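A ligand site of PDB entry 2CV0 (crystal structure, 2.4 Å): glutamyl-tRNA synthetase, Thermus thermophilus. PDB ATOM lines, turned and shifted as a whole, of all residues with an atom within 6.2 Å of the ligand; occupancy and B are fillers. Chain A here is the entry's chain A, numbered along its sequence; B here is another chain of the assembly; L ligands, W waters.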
ATOM      1  N   ARG A   5     -15.533   7.112 -20.563  1.00  0.00           N
ATOM      2  CA  ARG A   5     -16.115   5.947 -21.222  1.00  0.00           C
ATOM      3  C   ARG A   5     -16.345   6.096 -22.695  1.00  0.00           C
ATOM      4  O   ARG A   5     -16.384   7.209 -23.202  1.00  0.00           O
ATOM      5  CB  ARG A   5     -17.444   5.535 -20.582  1.00  0.00           C
ATOM      6  CG  ARG A   5     -18.502   6.619 -20.343  1.00  0.00           C
ATOM      7  CD  ARG A   5     -18.583   7.733 -21.348  1.00  0.00           C
ATOM      8  NE  ARG A   5     -19.866   8.450 -21.300  1.00  0.00           N
ATOM      9  CZ  ARG A   5     -20.343   9.106 -22.362  1.00  0.00           C
ATOM     10  NH1 ARG A   5     -19.607   9.097 -23.464  1.00  0.00           N
ATOM     11  NH2 ARG A   5     -21.528   9.699 -22.362  1.00  0.00           N
ATOM     12  N   ILE A   6     -16.454   4.961 -23.376  1.00  0.00           N
ATOM     13  CA  ILE A   6     -16.784   4.911 -24.782  1.00  0.00           C
ATOM     14  C   ILE A   6     -18.133   4.173 -24.706  1.00  0.00           C
ATOM     15  O   ILE A   6     -18.323   3.268 -23.885  1.00  0.00           O
ATOM     16  CB  ILE A   6     -15.719   4.117 -25.621  1.00  0.00           C
ATOM     17  CG1 ILE A   6     -16.082   4.163 -27.099  1.00  0.00           C
ATOM     18  CG2 ILE A   6     -15.661   2.675 -25.247  1.00  0.00           C
ATOM     19  CD1 ILE A   6     -16.244   5.565 -27.656  1.00  0.00           C
ATOM     20  N   ALA A   7     -19.114   4.577 -25.502  1.00  0.00           N
ATOM     21  CA  ALA A   7     -20.411   3.944 -25.406  1.00  0.00           C
ATOM     22  C   ALA A   7     -20.982   3.611 -26.783  1.00  0.00           C
ATOM     23  O   ALA A   7     -21.999   4.182 -27.207  1.00  0.00           O
ATOM     24  CB  ALA A   7     -21.370   4.828 -24.617  1.00  0.00           C
ATOM     25  N   PRO A   8     -20.352   2.667 -27.475  1.00  0.00           N
ATOM     26  CA  PRO A   8     -20.750   2.209 -28.816  1.00  0.00           C
ATOM     27  C   PRO A   8     -22.150   1.644 -28.845  1.00  0.00           C
ATOM     28  O   PRO A   8     -22.638   1.063 -27.866  1.00  0.00           O
ATOM     29  CB  PRO A   8     -19.728   1.129 -29.161  1.00  0.00           C
ATOM     30  CG  PRO A   8     -18.811   1.037 -27.973  1.00  0.00           C
ATOM     31  CD  PRO A   8     -19.453   1.707 -26.829  1.00  0.00           C
ATOM     32  N   SER A   9     -22.798   1.837 -29.991  1.00  0.00           N
ATOM     33  CA  SER A   9     -24.137   1.324 -30.239  1.00  0.00           C
ATOM     34  C   SER A   9     -23.873   0.145 -31.174  1.00  0.00           C
ATOM     35  O   SER A   9     -23.193   0.299 -32.170  1.00  0.00           O
ATOM     36  CB  SER A   9     -24.988   2.373 -30.945  1.00  0.00           C
ATOM     37  OG  SER A   9     -26.360   2.150 -30.751  1.00  0.00           O
ATOM     38  N   THR A  18     -15.576   5.435 -33.693  1.00  0.00           N
ATOM     39  CA  THR A  18     -15.590   4.898 -32.341  1.00  0.00           C
ATOM     40  C   THR A  18     -14.168   4.735 -31.821  1.00  0.00           C
ATOM     41  O   THR A  18     -13.885   5.105 -30.703  1.00  0.00           O
ATOM     42  CB  THR A  18     -16.272   3.518 -32.321  1.00  0.00           C
ATOM     43  OG1 THR A  18     -17.632   3.690 -32.681  1.00  0.00           O
ATOM     44  CG2 THR A  18     -16.194   2.870 -30.910  1.00  0.00           C
ATOM     45  N   ILE A  21     -12.744   8.220 -30.928  1.00  0.00           N
ATOM     46  CA  ILE A  21     -13.204   8.779 -29.662  1.00  0.00           C
ATOM     47  C   ILE A  21     -12.718   7.916 -28.471  1.00  0.00           C
ATOM     48  O   ILE A  21     -12.401   8.436 -27.404  1.00  0.00           O
ATOM     49  CB  ILE A  21     -14.750   8.875 -29.671  1.00  0.00           C
ATOM     50  CG1 ILE A  21     -15.203   9.925 -30.691  1.00  0.00           C
ATOM     51  CG2 ILE A  21     -15.275   9.256 -28.277  1.00  0.00           C
ATOM     52  CD1 ILE A  21     -14.734  11.347 -30.376  1.00  0.00           C
ATOM     53  N   ARG A  39     -19.457   0.899 -22.245  1.00  0.00           N
ATOM     54  CA  ARG A  39     -20.875   0.647 -21.954  1.00  0.00           C
ATOM     55  C   ARG A  39     -21.564   0.403 -23.283  1.00  0.00           C
ATOM     56  O   ARG A  39     -21.517   1.256 -24.149  1.00  0.00           O
ATOM     57  CB  ARG A  39     -21.545   1.846 -21.268  1.00  0.00           C
ATOM     58  CG  ARG A  39     -23.048   1.623 -20.997  1.00  0.00           C
ATOM     59  CD  ARG A  39     -23.659   2.750 -20.173  1.00  0.00           C
ATOM     60  NE  ARG A  39     -23.606   4.060 -20.823  1.00  0.00           N
ATOM     61  CZ  ARG A  39     -23.096   5.165 -20.274  1.00  0.00           C
ATOM     62  NH1 ARG A  39     -22.589   5.130 -19.053  1.00  0.00           N
ATOM     63  NH2 ARG A  39     -23.096   6.317 -20.942  1.00  0.00           N
ATOM     64  N   GLU A  41     -24.435   0.437 -25.694  1.00  0.00           N
ATOM     65  CA  GLU A  41     -25.699   1.169 -25.691  1.00  0.00           C
ATOM     66  C   GLU A  41     -26.693   0.587 -26.687  1.00  0.00           C
ATOM     67  O   GLU A  41     -26.971   1.159 -27.728  1.00  0.00           O
ATOM     68  CB  GLU A  41     -25.356   2.645 -25.996  1.00  0.00           C
ATOM     69  CG  GLU A  41     -26.052   3.651 -25.126  1.00  0.00           C
ATOM     70  CD  GLU A  41     -25.152   4.770 -24.619  1.00  0.00           C
ATOM     71  OE1 GLU A  41     -24.509   4.572 -23.563  1.00  0.00           O
ATOM     72  OE2 GLU A  41     -25.095   5.825 -25.277  1.00  0.00           O
ATOM     73  N   TYR A 187     -31.774   7.197 -25.881  1.00  0.00           N
ATOM     74  CA  TYR A 187     -30.382   7.512 -25.587  1.00  0.00           C
ATOM     75  C   TYR A 187     -30.223   8.614 -24.496  1.00  0.00           C
ATOM     76  O   TYR A 187     -29.369   8.515 -23.619  1.00  0.00           O
ATOM     77  CB  TYR A 187     -29.709   7.979 -26.885  1.00  0.00           C
ATOM     78  CG  TYR A 187     -28.484   8.803 -26.668  1.00  0.00           C
ATOM     79  CD1 TYR A 187     -27.265   8.201 -26.282  1.00  0.00           C
ATOM     80  CD2 TYR A 187     -28.548  10.202 -26.737  1.00  0.00           C
ATOM     81  CE1 TYR A 187     -26.147   8.977 -25.968  1.00  0.00           C
ATOM     82  CE2 TYR A 187     -27.438  10.982 -26.419  1.00  0.00           C
ATOM     83  CZ  TYR A 187     -26.247  10.369 -26.029  1.00  0.00           C
ATOM     84  OH  TYR A 187     -25.154  11.152 -25.677  1.00  0.00           O
ATOM     85  N   ASN A 191     -28.103   7.505 -21.080  1.00  0.00           N
ATOM     86  CA  ASN A 191     -26.783   8.089 -21.051  1.00  0.00           C
ATOM     87  C   ASN A 191     -26.540   8.834 -19.728  1.00  0.00           C
ATOM     88  O   ASN A 191     -25.482   8.691 -19.110  1.00  0.00           O
ATOM     89  CB  ASN A 191     -26.635   9.045 -22.240  1.00  0.00           C
ATOM     90  CG  ASN A 191     -25.185   9.323 -22.607  1.00  0.00           C
ATOM     91  OD1 ASN A 191     -24.694  10.432 -22.393  1.00  0.00           O
ATOM     92  ND2 ASN A 191     -24.502   8.318 -23.180  1.00  0.00           N
ATOM     93  N   ASP A 195     -24.112   7.281 -16.885  1.00  0.00           N
ATOM     94  CA  ASP A 195     -22.854   7.979 -16.631  1.00  0.00           C
ATOM     95  C   ASP A 195     -22.816   8.302 -15.140  1.00  0.00           C
ATOM     96  O   ASP A 195     -21.776   8.206 -14.487  1.00  0.00           O
ATOM     97  CB  ASP A 195     -22.752   9.293 -17.437  1.00  0.00           C
ATOM     98  CG  ASP A 195     -22.392   9.049 -18.905  1.00  0.00           C
ATOM     99  OD1 ASP A 195     -22.638   9.971 -19.724  1.00  0.00           O
ATOM    100  OD2 ASP A 195     -21.857   7.952 -19.243  1.00  0.00           O
ATOM    101  N   VAL A 203     -17.011  13.377 -19.925  1.00  0.00           N
ATOM    102  CA  VAL A 203     -17.635  12.911 -21.147  1.00  0.00           C
ATOM    103  C   VAL A 203     -16.913  13.484 -22.367  1.00  0.00           C
ATOM    104  O   VAL A 203     -17.022  14.679 -22.658  1.00  0.00           O
ATOM    105  CB  VAL A 203     -19.107  13.344 -21.192  1.00  0.00           C
ATOM    106  CG1 VAL A 203     -19.788  12.761 -22.452  1.00  0.00           C
ATOM    107  CG2 VAL A 203     -19.786  12.873 -19.924  1.00  0.00           C
ATOM    108  N   ILE A 204     -16.138  12.648 -23.060  1.00  0.00           N
ATOM    109  CA  ILE A 204     -15.421  13.085 -24.257  1.00  0.00           C
ATOM    110  C   ILE A 204     -16.170  12.354 -25.354  1.00  0.00           C
ATOM    111  O   ILE A 204     -16.274  11.119 -25.344  1.00  0.00           O
ATOM    112  CB  ILE A 204     -13.965  12.618 -24.250  1.00  0.00           C
ATOM    113  CG1 ILE A 204     -13.301  13.055 -22.937  1.00  0.00           C
ATOM    114  CG2 ILE A 204     -13.223  13.177 -25.448  1.00  0.00           C
ATOM    115  CD1 ILE A 204     -11.979  12.399 -22.717  1.00  0.00           C
ATOM    116  N   ARG A 205     -16.726  13.101 -26.286  1.00  0.00           N
ATOM    117  CA  ARG A 205     -17.495  12.484 -27.345  1.00  0.00           C
ATOM    118  C   ARG A 205     -17.458  13.371 -28.598  1.00  0.00           C
ATOM    119  O   ARG A 205     -16.949  14.492 -28.557  1.00  0.00           O
ATOM    120  CB  ARG A 205     -18.952  12.285 -26.868  1.00  0.00           C
ATOM    121  CG  ARG A 205     -19.844  13.452 -27.189  1.00  0.00           C
ATOM    122  CD  ARG A 205     -20.548  14.068 -25.998  1.00  0.00           C
ATOM    123  NE  ARG A 205     -21.561  13.207 -25.402  1.00  0.00           N
ATOM    124  CZ  ARG A 205     -22.628  13.672 -24.733  1.00  0.00           C
ATOM    125  NH1 ARG A 205     -22.838  14.962 -24.592  1.00  0.00           N
ATOM    126  NH2 ARG A 205     -23.463  12.814 -24.160  1.00  0.00           N
ATOM    127  N   ALA A 206     -18.014  12.871 -29.698  1.00  0.00           N
ATOM    128  CA  ALA A 206     -17.982  13.587 -30.940  1.00  0.00           C
ATOM    129  C   ALA A 206     -18.928  14.768 -30.916  1.00  0.00           C
ATOM    130  O   ALA A 206     -20.012  14.712 -30.318  1.00  0.00           O
ATOM    131  CB  ALA A 206     -18.327  12.653 -32.104  1.00  0.00           C
ATOM    132  N   GLU A 208     -21.009  15.780 -32.862  1.00  0.00           N
ATOM    133  CA  GLU A 208     -22.417  15.553 -33.237  1.00  0.00           C
ATOM    134  C   GLU A 208     -23.364  15.555 -32.034  1.00  0.00           C
ATOM    135  O   GLU A 208     -24.567  15.693 -32.208  1.00  0.00           O
ATOM    136  CB  GLU A 208     -22.583  14.245 -34.015  1.00  0.00           C
ATOM    137  CG  GLU A 208     -22.368  12.977 -33.186  1.00  0.00           C
ATOM    138  CD  GLU A 208     -22.567  11.725 -34.025  1.00  0.00           C
ATOM    139  OE1 GLU A 208     -23.709  11.446 -34.464  1.00  0.00           O
ATOM    140  OE2 GLU A 208     -21.560  11.006 -34.236  1.00  0.00           O
ATOM    141  N   TRP A 209     -22.829  15.410 -30.821  1.00  0.00           N
ATOM    142  CA  TRP A 209     -23.628  15.394 -29.589  1.00  0.00           C
ATOM    143  C   TRP A 209     -23.719  16.748 -28.856  1.00  0.00           C
ATOM    144  O   TRP A 209     -24.455  16.866 -27.866  1.00  0.00           O
ATOM    145  CB  TRP A 209     -23.064  14.359 -28.610  1.00  0.00           C
ATOM    146  CG  TRP A 209     -23.020  13.005 -29.165  1.00  0.00           C
ATOM    147  CD1 TRP A 209     -21.910  12.349 -29.621  1.00  0.00           C
ATOM    148  CD2 TRP A 209     -24.117  12.155 -29.424  1.00  0.00           C
ATOM    149  NE1 TRP A 209     -22.260  11.151 -30.162  1.00  0.00           N
ATOM    150  CE2 TRP A 209     -23.619  11.002 -30.054  1.00  0.00           C
ATOM    151  CE3 TRP A 209     -25.501  12.261 -29.191  1.00  0.00           C
ATOM    152  CZ2 TRP A 209     -24.448   9.944 -30.451  1.00  0.00           C
ATOM    153  CZ3 TRP A 209     -26.318  11.220 -29.583  1.00  0.00           C
ATOM    154  CH2 TRP A 209     -25.787  10.077 -30.209  1.00  0.00           C
ATOM    155  N   HIS A 216     -29.119  16.955 -21.672  1.00  0.00           N
ATOM    156  CA  HIS A 216     -28.484  16.235 -20.565  1.00  0.00           C
ATOM    157  C   HIS A 216     -28.236  17.086 -19.300  1.00  0.00           C
ATOM    158  O   HIS A 216     -28.392  16.590 -18.178  1.00  0.00           O
ATOM    159  CB  HIS A 216     -27.210  15.623 -21.081  1.00  0.00           C
ATOM    160  CG  HIS A 216     -27.443  14.779 -22.285  1.00  0.00           C
ATOM    161  ND1 HIS A 216     -26.470  14.515 -23.219  1.00  0.00           N
ATOM    162  CD2 HIS A 216     -28.567  14.184 -22.742  1.00  0.00           C
ATOM    163  CE1 HIS A 216     -26.984  13.805 -24.198  1.00  0.00           C
ATOM    164  NE2 HIS A 216     -28.259  13.590 -23.932  1.00  0.00           N
ATOM    165  P     A B  75     -32.218   5.299 -29.326  1.00  0.00           P
ATOM    166  OP1   A B  75     -32.766   4.368 -28.297  1.00  0.00           O
ATOM    167  OP2   A B  75     -32.015   6.724 -28.972  1.00  0.00           O
ATOM    168  O5'   A B  75     -30.879   4.623 -29.870  1.00  0.00           O
ATOM    169  C5'   A B  75     -29.698   4.631 -29.135  1.00  0.00           C
ATOM    170  C4'   A B  75     -28.511   4.856 -30.045  1.00  0.00           C
ATOM    171  O4'   A B  75     -28.906   5.549 -31.258  1.00  0.00           O
ATOM    172  C3'   A B  75     -27.511   5.775 -29.369  1.00  0.00           C
ATOM    173  O3'   A B  75     -26.892   4.974 -28.370  1.00  0.00           O
ATOM    174  C2'   A B  75     -26.805   6.426 -30.555  1.00  0.00           C
ATOM    175  O2'   A B  75     -25.782   5.632 -31.102  1.00  0.00           O
ATOM    176  C1'   A B  75     -27.974   6.590 -31.547  1.00  0.00           C
ATOM    177  N9    A B  75     -28.643   7.887 -31.393  1.00  0.00           N
ATOM    178  C8    A B  75     -29.742   8.177 -30.627  1.00  0.00           C
ATOM    179  N7    A B  75     -30.065   9.451 -30.618  1.00  0.00           N
ATOM    180  C5    A B  75     -29.116  10.037 -31.449  1.00  0.00           C
ATOM    181  C6    A B  75     -28.869  11.386 -31.806  1.00  0.00           C
ATOM    182  N6    A B  75     -29.571  12.413 -31.326  1.00  0.00           N
ATOM    183  N1    A B  75     -27.848  11.635 -32.653  1.00  0.00           N
ATOM    184  C2    A B  75     -27.113  10.603 -33.095  1.00  0.00           C
ATOM    185  N3    A B  75     -27.238   9.301 -32.808  1.00  0.00           N
ATOM    186  C4    A B  75     -28.257   9.084 -31.962  1.00  0.00           C
HETATM  187  N1  LIG L   1     -24.402   5.784 -27.896  1.00  0.00           N
HETATM  188  C1  LIG L   1     -23.820   7.098 -28.218  1.00  0.00           C
HETATM  189  C2  LIG L   1     -23.006   6.937 -29.486  1.00  0.00           C
HETATM  190  O1  LIG L   1     -23.604   7.021 -30.582  1.00  0.00           O
HETATM  191  C3  LIG L   1     -22.936   7.584 -27.044  1.00  0.00           C
HETATM  192  C4  LIG L   1     -22.315   8.961 -27.248  1.00  0.00           C
HETATM  193  C5  LIG L   1     -21.948   9.634 -25.930  1.00  0.00           C
HETATM  194  O2  LIG L   1     -22.816  10.271 -25.268  1.00  0.00           O
HETATM  195  O3  LIG L   1     -20.787   9.491 -25.546  1.00  0.00           O
HETATM  196  O4  LIG L   1     -21.783   6.722 -29.384  1.00  0.00           O
HETATM  197  O   HOH W   1     -19.419   6.398 -27.807  1.00  0.00           O
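ND2 of Asn 191 sits at hydrogen-bond distance from O2 of the ligand, 3.3 Å away.
N1 of the ligand sits at hydrogen-bond distance from O3' of A 75 of chain B.
N1 of the ligand lies within salt-bridge range of OE2 of Glu 41, at 2.7 Å.
NH1 of Arg 5 lies within salt-bridge range of O3 of the ligand, at 2.4 Å.
NH2 of Arg 205 lies within salt-bridge range of O2 of the ligand, 2.8 Å away.
The side-chain hydroxyl (OH) of Tyr 187 lies within hydrogen-bond range of an oxygen (O2) of the ligand (2.5 Å).
The backbone carbonyl oxygen of Ala 7 is in hydrogen-bond range of a nitrogen (N1) of the ligand, at 3.0 Å.
Trp 209 touches the ligand.
Hydrophobic or aromatic side chains within 4 Å of the ligand: Ala 7, Tyr 187 and Trp 209.
Within 4 Å of the ligand: Arg 5, Ala 7, Glu 41, Tyr 187, Asn 191, Arg 205, Trp 209 and A 75 of chain B.
Along chain A the residues within 4 Å of the ligand span positions 5 to 209.
Water W1 lies within hydrogen-bond range of O4 of the ligand and N of Ala 7.
OD1 of Asp 195 lies close to OD1 of Asn 191 (3.4 Å).
The guanidinium group (NH2) of Arg 205 sits at hydrogen-bond distance from the side-chain amide oxygen (OD1) of Asn 191 (3.2 Å).
The guanidinium group of Arg 5 is in salt-bridge range of the side-chain carboxylate of Asp 195 (2.9 Å).
The side-chain hydroxyl of Tyr 187 lies within hydrogen-bond range of the guanidinium group of Arg 205, at 2.8 Å.
The side-chain carboxylate of Glu 41 lies within salt-bridge range of the guanidinium group of Arg 39 (2.9 Å).
NH2 of Arg 5 is in hydrogen-bond range of OD1 of Asn 191 (3.2 Å).
The side-chain carboxylate (OE2) of Glu 41 is in hydrogen-bond range of the side-chain amide nitrogen (ND2) of Asn 191, at 3.3 Å.
The backbone carbonyl oxygen (O) of Glu 41 lies within hydrogen-bond range of the side-chain hydroxyl (OG) of Ser 9 (3.2 Å).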
